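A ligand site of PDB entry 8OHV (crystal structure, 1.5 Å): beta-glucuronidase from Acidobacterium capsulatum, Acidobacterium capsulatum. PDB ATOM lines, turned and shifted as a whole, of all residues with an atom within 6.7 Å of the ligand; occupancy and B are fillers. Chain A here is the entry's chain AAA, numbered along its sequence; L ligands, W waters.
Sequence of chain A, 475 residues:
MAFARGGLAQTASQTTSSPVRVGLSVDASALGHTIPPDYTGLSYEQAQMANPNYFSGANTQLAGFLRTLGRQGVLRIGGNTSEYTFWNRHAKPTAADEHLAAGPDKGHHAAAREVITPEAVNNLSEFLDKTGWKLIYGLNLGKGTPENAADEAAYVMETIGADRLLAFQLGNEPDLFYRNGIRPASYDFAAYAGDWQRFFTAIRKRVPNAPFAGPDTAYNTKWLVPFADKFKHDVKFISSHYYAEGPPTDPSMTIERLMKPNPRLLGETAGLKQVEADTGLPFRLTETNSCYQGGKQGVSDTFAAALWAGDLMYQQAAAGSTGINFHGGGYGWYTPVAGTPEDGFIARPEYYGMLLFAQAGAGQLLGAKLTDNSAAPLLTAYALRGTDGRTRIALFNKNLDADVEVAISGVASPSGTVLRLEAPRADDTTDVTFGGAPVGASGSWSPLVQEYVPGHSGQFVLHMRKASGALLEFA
Water W2 lies within hydrogen-bond range of an oxygen (O1) of the ligand (2.9 Å) and the side-chain amide nitrogen of Asn 80 (3.0 Å).
OE2 of Glu 287 is in salt-bridge range of N1 of the ligand.
OH of Tyr 334 sits at hydrogen-bond distance from O2 of the ligand, 2.6 Å away.
OE2 of Glu 45 is in hydrogen-bond range of O4 of the ligand, at 2.7 Å.
O5 of the ligand sits at hydrogen-bond distance from N of Asp 105, 3.2 Å away.
The backbone carbonyl oxygen (O) of Asp 105 lies within hydrogen-bond range of an oxygen (O5) of the ligand (2.7 Å).
N of Gln 293 sits at hydrogen-bond distance from O1 of the ligand, 2.8 Å away.
N of Asn 80 sits at hydrogen-bond distance from O4 of the ligand (2.8 Å).
The side-chain amide nitrogen (ND2) of Asn 80 lies close to an oxygen (O4) of the ligand.
O3 of the ligand is in hydrogen-bond range of NE2 of His 327, at 2.9 Å.
A nitrogen (N1) of the ligand lies within salt-bridge range of the side-chain carboxylate (OE2) of Glu 173 (2.9 Å).
N of Gly 294 lies within hydrogen-bond range of O2 of the ligand, 3.0 Å away.
CA of Gly 79 touches O4 of the ligand (3.6 Å).
Pro 104 touches the ligand.
Tyr 243 touches the ligand (OH to C6, 3.6 Å).
Tyr 292 touches the ligand (CB to O1, 3.5 Å).
Hydrophobic or aromatic side chains within 4 Å of the ligand: Pro 104, Tyr 243, Tyr 292, His 327 and Tyr 334.
Within 4 Å of the ligand: Glu 45, Gly 79, Asn 80, Pro 104, Asp 105, Glu 173, Tyr 243, Glu 287, Tyr 292, Gln 293, Gly 294, His 327 and Tyr 334.
The nearest printed residue that does not touch the ligand is Asn 172 (4.1 Å).
The guanidinium group (NH1) of Arg 76 lies within salt-bridge range of the side-chain carboxylate (OE1) of Glu 287, at 2.8 Å.
The side-chain hydroxyl (OH) of Tyr 243 is in hydrogen-bond range of the side-chain hydroxyl (OH) of Tyr 334 (3.5 Å).
OE1 of Glu 45 sits at hydrogen-bond distance from N of Asn 80 (3.4 Å).
OD2 of Asp 105 sits at hydrogen-bond distance from ND2 of Asn 80, at 2.9 Å.
OD2 of Asp 105 lies within hydrogen-bond range of N of Gly 107, 2.9 Å away.
The side-chain amide nitrogen (NE2) of Gln 293 sits at hydrogen-bond distance from the side-chain hydroxyl (OH) of Tyr 292, 3.1 Å away.
ND1 of His 327 sits at hydrogen-bond distance from OG of Ser 43, 2.7 Å away.
A ring nitrogen (ND1) of His 241 is in hydrogen-bond range of the side-chain carboxylate (OE2) of Glu 173 (2.7 Å).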
ATOM      1  N   SER A  43      -3.737 -17.374   5.585  1.00  0.00           N
ATOM      2  CA  SER A  43      -4.531 -17.357   4.352  1.00  0.00           C
ATOM      3  C   SER A  43      -3.842 -18.175   3.259  1.00  0.00           C
ATOM      4  O   SER A  43      -2.605 -18.158   3.192  1.00  0.00           O
ATOM      5  CB  SER A  43      -4.721 -15.929   3.895  1.00  0.00           C
ATOM      6  OG  SER A  43      -5.276 -15.900   2.635  1.00  0.00           O
ATOM      7  N   GLU A  45      -4.495 -19.801  -0.987  1.00  0.00           N
ATOM      8  CA  GLU A  45      -5.276 -19.793  -2.264  1.00  0.00           C
ATOM      9  C   GLU A  45      -6.324 -20.910  -2.294  1.00  0.00           C
ATOM     10  O   GLU A  45      -6.029 -22.072  -1.934  1.00  0.00           O
ATOM     11  CB  GLU A  45      -4.298 -19.968  -3.432  1.00  0.00           C
ATOM     12  CG  GLU A  45      -3.379 -18.766  -3.664  1.00  0.00           C
ATOM     13  CD  GLU A  45      -4.023 -17.501  -4.140  1.00  0.00           C
ATOM     14  OE1 GLU A  45      -5.229 -17.525  -4.602  1.00  0.00           O
ATOM     15  OE2 GLU A  45      -3.365 -16.434  -3.959  1.00  0.00           O
ATOM     16  N   ARG A  76      -8.029 -18.926   6.502  1.00  0.00           N
ATOM     17  CA  ARG A  76      -8.843 -18.282   5.467  1.00  0.00           C
ATOM     18  C   ARG A  76      -8.438 -18.888   4.144  1.00  0.00           C
ATOM     19  O   ARG A  76      -7.183 -18.942   3.881  1.00  0.00           O
ATOM     20  CB  ARG A  76      -8.651 -16.760   5.515  1.00  0.00           C
ATOM     21  CG  ARG A  76      -9.438 -16.025   4.432  1.00  0.00           C
ATOM     22  CD  ARG A  76      -8.513 -15.655   3.291  1.00  0.00           C
ATOM     23  NE  ARG A  76      -9.179 -14.886   2.264  1.00  0.00           N
ATOM     24  CZ  ARG A  76      -8.520 -14.319   1.252  1.00  0.00           C
ATOM     25  NH1 ARG A  76      -7.195 -14.431   1.194  1.00  0.00           N
ATOM     26  NH2 ARG A  76      -9.214 -13.656   0.344  1.00  0.00           N
ATOM     27  N   GLY A  78      -9.061 -18.297   0.073  1.00  0.00           N
ATOM     28  CA  GLY A  78      -9.585 -17.291  -0.864  1.00  0.00           C
ATOM     29  C   GLY A  78      -8.571 -16.924  -1.927  1.00  0.00           C
ATOM     30  O   GLY A  78      -8.057 -17.765  -2.651  1.00  0.00           O
ATOM     31  N   GLY A  79      -8.328 -15.641  -2.014  1.00  0.00           N
ATOM     32  CA  GLY A  79      -7.288 -15.106  -2.916  1.00  0.00           C
ATOM     33  C   GLY A  79      -7.772 -15.064  -4.359  1.00  0.00           C
ATOM     34  O   GLY A  79      -8.951 -15.360  -4.671  1.00  0.00           O
ATOM     35  N   ASN A  80      -6.871 -14.660  -5.255  1.00  0.00           N
ATOM     36  CA  ASN A  80      -7.195 -14.459  -6.668  1.00  0.00           C
ATOM     37  C   ASN A  80      -7.725 -15.764  -7.247  1.00  0.00           C
ATOM     38  O   ASN A  80      -8.609 -15.706  -8.144  1.00  0.00           O
ATOM     39  CB  ASN A  80      -5.968 -14.004  -7.447  1.00  0.00           C
ATOM     40  CG  ASN A  80      -5.545 -12.595  -7.132  1.00  0.00           C
ATOM     41  OD1 ASN A  80      -6.319 -11.829  -6.532  1.00  0.00           O
ATOM     42  ND2 ASN A  80      -4.277 -12.285  -7.488  1.00  0.00           N
ATOM     43  N   THR A  81      -7.223 -16.893  -6.796  1.00  0.00           N
ATOM     44  CA  THR A  81      -7.653 -18.185  -7.403  1.00  0.00           C
ATOM     45  C   THR A  81      -9.096 -18.496  -7.041  1.00  0.00           C
ATOM     46  O   THR A  81      -9.669 -19.419  -7.678  1.00  0.00           O
ATOM     47  CB  THR A  81      -6.734 -19.345  -7.052  1.00  0.00           C
ATOM     48  OG1 THR A  81      -6.781 -19.577  -5.645  1.00  0.00           O
ATOM     49  CG2 THR A  81      -5.313 -19.130  -7.524  1.00  0.00           C
ATOM     50  N   GLY A 103       0.940 -22.023  -4.536  1.00  0.00           N
ATOM     51  CA  GLY A 103       1.485 -20.850  -3.829  1.00  0.00           C
ATOM     52  C   GLY A 103       0.653 -19.610  -4.155  1.00  0.00           C
ATOM     53  O   GLY A 103      -0.266 -19.637  -4.989  1.00  0.00           O
ATOM     54  N   PRO A 104       0.946 -18.499  -3.459  1.00  0.00           N
ATOM     55  CA  PRO A 104       0.253 -17.243  -3.682  1.00  0.00           C
ATOM     56  C   PRO A 104       0.255 -16.918  -5.167  1.00  0.00           C
ATOM     57  O   PRO A 104       1.270 -16.987  -5.830  1.00  0.00           O
ATOM     58  CB  PRO A 104       1.052 -16.208  -2.889  1.00  0.00           C
ATOM     59  CG  PRO A 104       1.665 -17.035  -1.810  1.00  0.00           C
ATOM     60  CD  PRO A 104       1.981 -18.375  -2.432  1.00  0.00           C
ATOM     61  N   ASP A 105      -0.912 -16.510  -5.636  1.00  0.00           N
ATOM     62  CA  ASP A 105      -1.070 -16.038  -7.030  1.00  0.00           C
ATOM     63  C   ASP A 105      -0.236 -14.784  -7.253  1.00  0.00           C
ATOM     64  O   ASP A 105      -0.243 -13.887  -6.399  1.00  0.00           O
ATOM     65  CB  ASP A 105      -2.566 -15.800  -7.301  1.00  0.00           C
ATOM     66  CG  ASP A 105      -2.805 -15.469  -8.773  1.00  0.00           C
ATOM     67  OD1 ASP A 105      -2.886 -16.420  -9.587  1.00  0.00           O
ATOM     68  OD2 ASP A 105      -2.900 -14.280  -9.063  1.00  0.00           O
ATOM     69  N   LYS A 106       0.442 -14.702  -8.407  1.00  0.00           N
ATOM     70  CA  LYS A 106       1.341 -13.554  -8.626  1.00  0.00           C
ATOM     71  C   LYS A 106       0.612 -12.379  -9.262  1.00  0.00           C
ATOM     72  O   LYS A 106       1.253 -11.313  -9.342  1.00  0.00           O
ATOM     73  CB  LYS A 106       2.563 -13.990  -9.441  1.00  0.00           C
ATOM     74  CG  LYS A 106       3.416 -15.049  -8.747  1.00  0.00           C
ATOM     75  CD  LYS A 106       4.740 -15.274  -9.484  1.00  0.00           C
ATOM     76  CE  LYS A 106       5.689 -16.217  -8.772  1.00  0.00           C
ATOM     77  NZ  LYS A 106       5.055 -17.527  -8.553  1.00  0.00           N
ATOM     78  N   GLY A 107      -0.657 -12.538  -9.660  1.00  0.00           N
ATOM     79  CA  GLY A 107      -1.557 -11.438 -10.043  1.00  0.00           C
ATOM     80  C   GLY A 107      -1.139 -10.786 -11.365  1.00  0.00           C
ATOM     81  O   GLY A 107      -1.482  -9.594 -11.578  1.00  0.00           O
ATOM     82  N   ASN A 172     -13.014 -12.274  -3.742  1.00  0.00           N
ATOM     83  CA  ASN A 172     -11.734 -11.798  -3.183  1.00  0.00           C
ATOM     84  C   ASN A 172     -11.400 -10.485  -3.894  1.00  0.00           C
ATOM     85  O   ASN A 172     -11.517 -10.458  -5.133  1.00  0.00           O
ATOM     86  CB  ASN A 172     -10.655 -12.830  -3.479  1.00  0.00           C
ATOM     87  CG  ASN A 172      -9.268 -12.282  -3.316  1.00  0.00           C
ATOM     88  OD1 ASN A 172      -8.756 -12.178  -2.211  1.00  0.00           O
ATOM     89  ND2 ASN A 172      -8.636 -11.932  -4.447  1.00  0.00           N
ATOM     90  N   GLU A 173     -11.049  -9.425  -3.148  1.00  0.00           N
ATOM     91  CA  GLU A 173     -10.590  -8.137  -3.771  1.00  0.00           C
ATOM     92  C   GLU A 173     -11.536  -7.696  -4.889  1.00  0.00           C
ATOM     93  O   GLU A 173     -11.093  -7.404  -6.014  1.00  0.00           O
ATOM     94  CB  GLU A 173      -9.151  -8.338  -4.226  1.00  0.00           C
ATOM     95  CG  GLU A 173      -8.225  -8.610  -3.050  1.00  0.00           C
ATOM     96  CD  GLU A 173      -6.729  -8.678  -3.305  1.00  0.00           C
ATOM     97  OE1 GLU A 173      -6.311  -8.711  -4.464  1.00  0.00           O
ATOM     98  OE2 GLU A 173      -5.964  -8.639  -2.331  1.00  0.00           O
ATOM     99  N   ALA A 218      -8.905  -5.418  -1.568  1.00  0.00           N
ATOM    100  CA  ALA A 218      -7.438  -5.310  -1.664  1.00  0.00           C
ATOM    101  C   ALA A 218      -6.958  -4.048  -0.963  1.00  0.00           C
ATOM    102  O   ALA A 218      -5.917  -4.121  -0.278  1.00  0.00           O
ATOM    103  CB  ALA A 218      -7.003  -5.248  -3.097  1.00  0.00           C
ATOM    104  N   HIS A 241      -7.671  -6.193   3.211  1.00  0.00           N
ATOM    105  CA  HIS A 241      -6.318  -6.770   2.989  1.00  0.00           C
ATOM    106  C   HIS A 241      -5.264  -5.679   3.210  1.00  0.00           C
ATOM    107  O   HIS A 241      -5.583  -4.458   3.273  1.00  0.00           O
ATOM    108  CB  HIS A 241      -6.183  -7.361   1.590  1.00  0.00           C
ATOM    109  CG  HIS A 241      -7.119  -8.483   1.323  1.00  0.00           C
ATOM    110  ND1 HIS A 241      -7.180  -9.094   0.074  1.00  0.00           N
ATOM    111  CD2 HIS A 241      -8.057  -9.097   2.085  1.00  0.00           C
ATOM    112  CE1 HIS A 241      -8.049 -10.088   0.147  1.00  0.00           C
ATOM    113  NE2 HIS A 241      -8.639 -10.115   1.360  1.00  0.00           N
ATOM    114  N   TYR A 243      -0.943  -5.091   2.009  1.00  0.00           N
ATOM    115  CA  TYR A 243       0.455  -5.424   1.588  1.00  0.00           C
ATOM    116  C   TYR A 243       1.328  -4.174   1.745  1.00  0.00           C
ATOM    117  O   TYR A 243       0.962  -3.170   1.185  1.00  0.00           O
ATOM    118  CB  TYR A 243       0.519  -5.973   0.167  1.00  0.00           C
ATOM    119  CG  TYR A 243      -0.019  -7.376   0.061  1.00  0.00           C
ATOM    120  CD1 TYR A 243      -1.373  -7.612   0.065  1.00  0.00           C
ATOM    121  CD2 TYR A 243       0.832  -8.456   0.201  1.00  0.00           C
ATOM    122  CE1 TYR A 243      -1.886  -8.905   0.110  1.00  0.00           C
ATOM    123  CE2 TYR A 243       0.362  -9.758   0.257  1.00  0.00           C
ATOM    124  CZ  TYR A 243      -1.008  -9.968   0.192  1.00  0.00           C
ATOM    125  OH  TYR A 243      -1.463 -11.264   0.246  1.00  0.00           O
ATOM    126  N   GLU A 287      -6.327 -10.929   4.798  1.00  0.00           N
ATOM    127  CA  GLU A 287      -5.188 -11.315   3.920  1.00  0.00           C
ATOM    128  C   GLU A 287      -4.119 -10.244   3.961  1.00  0.00           C
ATOM    129  O   GLU A 287      -4.411  -9.067   3.658  1.00  0.00           O
ATOM    130  CB  GLU A 287      -5.656 -11.515   2.466  1.00  0.00           C
ATOM    131  CG  GLU A 287      -4.641 -12.314   1.674  1.00  0.00           C
ATOM    132  CD  GLU A 287      -4.775 -12.154   0.193  1.00  0.00           C
ATOM    133  OE1 GLU A 287      -5.685 -12.782  -0.439  1.00  0.00           O
ATOM    134  OE2 GLU A 287      -4.064 -11.267  -0.297  1.00  0.00           O
ATOM    135  N   ASN A 289       0.431  -9.613   3.659  1.00  0.00           N
ATOM    136  CA  ASN A 289       1.855 -10.032   3.736  1.00  0.00           C
ATOM    137  C   ASN A 289       2.714  -8.879   3.223  1.00  0.00           C
ATOM    138  O   ASN A 289       2.212  -7.756   3.020  1.00  0.00           O
ATOM    139  CB  ASN A 289       2.133 -11.383   3.046  1.00  0.00           C
ATOM    140  CG  ASN A 289       3.079 -12.182   3.900  1.00  0.00           C
ATOM    141  OD1 ASN A 289       4.050 -11.602   4.390  1.00  0.00           O
ATOM    142  ND2 ASN A 289       2.766 -13.463   4.199  1.00  0.00           N
ATOM    143  N   CYS A 291       4.893  -8.026   0.634  1.00  0.00           N
ATOM    144  CA  CYS A 291       4.995  -7.479  -0.736  1.00  0.00           C
ATOM    145  C   CYS A 291       4.066  -8.263  -1.643  1.00  0.00           C
ATOM    146  O   CYS A 291       4.099  -9.474  -1.583  1.00  0.00           O
ATOM    147  CB  CYS A 291       6.442  -7.586  -1.216  1.00  0.00           C
ATOM    148  SG  CYS A 291       7.642  -6.800  -0.104  1.00  0.00           S
ATOM    149  N   TYR A 292       3.220  -7.581  -2.432  1.00  0.00           N
ATOM    150  CA  TYR A 292       2.256  -8.269  -3.325  1.00  0.00           C
ATOM    151  C   TYR A 292       2.963  -8.859  -4.559  1.00  0.00           C
ATOM    152  O   TYR A 292       4.211  -8.916  -4.658  1.00  0.00           O
ATOM    153  CB  TYR A 292       1.087  -7.354  -3.637  1.00  0.00           C
ATOM    154  CG  TYR A 292       1.247  -6.418  -4.819  1.00  0.00           C
ATOM    155  CD1 TYR A 292       0.169  -6.201  -5.672  1.00  0.00           C
ATOM    156  CD2 TYR A 292       2.444  -5.809  -5.120  1.00  0.00           C
ATOM    157  CE1 TYR A 292       0.269  -5.344  -6.752  1.00  0.00           C
ATOM    158  CE2 TYR A 292       2.572  -4.944  -6.196  1.00  0.00           C
ATOM    159  CZ  TYR A 292       1.476  -4.706  -7.011  1.00  0.00           C
ATOM    160  OH  TYR A 292       1.586  -3.872  -8.079  1.00  0.00           O
ATOM    161  N   GLN A 293       2.178  -9.449  -5.442  1.00  0.00           N
ATOM    162  CA  GLN A 293       2.651 -10.244  -6.594  1.00  0.00           C
ATOM    163  C   GLN A 293       3.528 -11.402  -6.090  1.00  0.00           C
ATOM    164  O   GLN A 293       4.490 -11.753  -6.746  1.00  0.00           O
ATOM    165  CB  GLN A 293       3.271  -9.290  -7.642  1.00  0.00           C
ATOM    166  CG  GLN A 293       2.174  -8.379  -8.237  1.00  0.00           C
ATOM    167  CD  GLN A 293       2.649  -7.361  -9.250  1.00  0.00           C
ATOM    168  OE1 GLN A 293       3.815  -7.312  -9.615  1.00  0.00           O
ATOM    169  NE2 GLN A 293       1.728  -6.548  -9.729  1.00  0.00           N
ATOM    170  N   GLY A 294       3.190 -11.973  -4.914  1.00  0.00           N
ATOM    171  CA  GLY A 294       3.836 -13.189  -4.379  1.00  0.00           C
ATOM    172  C   GLY A 294       5.096 -12.905  -3.578  1.00  0.00           C
ATOM    173  O   GLY A 294       5.704 -13.875  -3.150  1.00  0.00           O
ATOM    174  N   GLY A 295       5.447 -11.660  -3.327  1.00  0.00           N
ATOM    175  CA  GLY A 295       6.598 -11.351  -2.480  1.00  0.00           C
ATOM    176  C   GLY A 295       7.860 -11.050  -3.268  1.00  0.00           C
ATOM    177  O   GLY A 295       7.915 -11.260  -4.503  1.00  0.00           O
ATOM    178  N   HIS A 327      -0.996 -14.392   4.338  1.00  0.00           N
ATOM    179  CA  HIS A 327      -1.117 -15.182   3.115  1.00  0.00           C
ATOM    180  C   HIS A 327       0.137 -15.989   2.828  1.00  0.00           C
ATOM    181  O   HIS A 327       1.245 -15.650   3.233  1.00  0.00           O
ATOM    182  CB  HIS A 327      -1.467 -14.251   1.919  1.00  0.00           C
ATOM    183  CG  HIS A 327      -2.056 -15.037   0.792  1.00  0.00           C
ATOM    184  ND1 HIS A 327      -3.245 -15.753   0.903  1.00  0.00           N
ATOM    185  CD2 HIS A 327      -1.692 -15.096  -0.498  1.00  0.00           C
ATOM    186  CE1 HIS A 327      -3.502 -16.335  -0.250  1.00  0.00           C
ATOM    187  NE2 HIS A 327      -2.602 -15.889  -1.180  1.00  0.00           N
ATOM    188  N   TYR A 334       6.806 -15.002   0.539  1.00  0.00           N
ATOM    189  CA  TYR A 334       6.326 -14.516   1.849  1.00  0.00           C
ATOM    190  C   TYR A 334       5.614 -15.573   2.738  1.00  0.00           C
ATOM    191  O   TYR A 334       5.105 -15.229   3.810  1.00  0.00           O
ATOM    192  CB  TYR A 334       5.500 -13.245   1.722  1.00  0.00           C
ATOM    193  CG  TYR A 334       4.258 -13.275   0.858  1.00  0.00           C
ATOM    194  CD1 TYR A 334       3.244 -14.204   1.067  1.00  0.00           C
ATOM    195  CD2 TYR A 334       4.096 -12.357  -0.155  1.00  0.00           C
ATOM    196  CE1 TYR A 334       2.112 -14.242   0.272  1.00  0.00           C
ATOM    197  CE2 TYR A 334       2.934 -12.335  -0.910  1.00  0.00           C
ATOM    198  CZ  TYR A 334       1.988 -13.315  -0.758  1.00  0.00           C
ATOM    199  OH  TYR A 334       0.827 -13.260  -1.469  1.00  0.00           O
HETATM  200  C1  LIG L   1      -4.582 -11.710  -3.667  1.00  0.00           C
HETATM  201  C2  LIG L   1      -3.728 -12.974  -3.649  1.00  0.00           C
HETATM  202  C3  LIG L   1      -2.302 -12.638  -4.109  1.00  0.00           C
HETATM  203  N1  LIG L   1      -3.965 -10.654  -2.822  1.00  0.00           N
HETATM  204  C4  LIG L   1      -2.631 -10.270  -3.308  1.00  0.00           C
HETATM  205  O1  LIG L   1      -0.399 -10.292  -4.837  1.00  0.00           O
HETATM  206  C5  LIG L   1      -0.362 -11.093  -3.900  1.00  0.00           C
HETATM  207  O2  LIG L   1       0.689 -11.488  -3.372  1.00  0.00           O
HETATM  208  C6  LIG L   1      -1.695 -11.477  -3.301  1.00  0.00           C
HETATM  209  O3  LIG L   1      -3.620 -13.459  -2.315  1.00  0.00           O
HETATM  210  O4  LIG L   1      -4.292 -13.987  -4.461  1.00  0.00           O
HETATM  211  O5  LIG L   1      -1.492 -13.800  -3.990  1.00  0.00           O
HETATM  212  O   HOH W   1      -3.876  -7.835  -5.482  1.00  0.00           O
HETATM  213  O   HOH W   2      -2.472  -9.935  -6.872  1.00  0.00           O
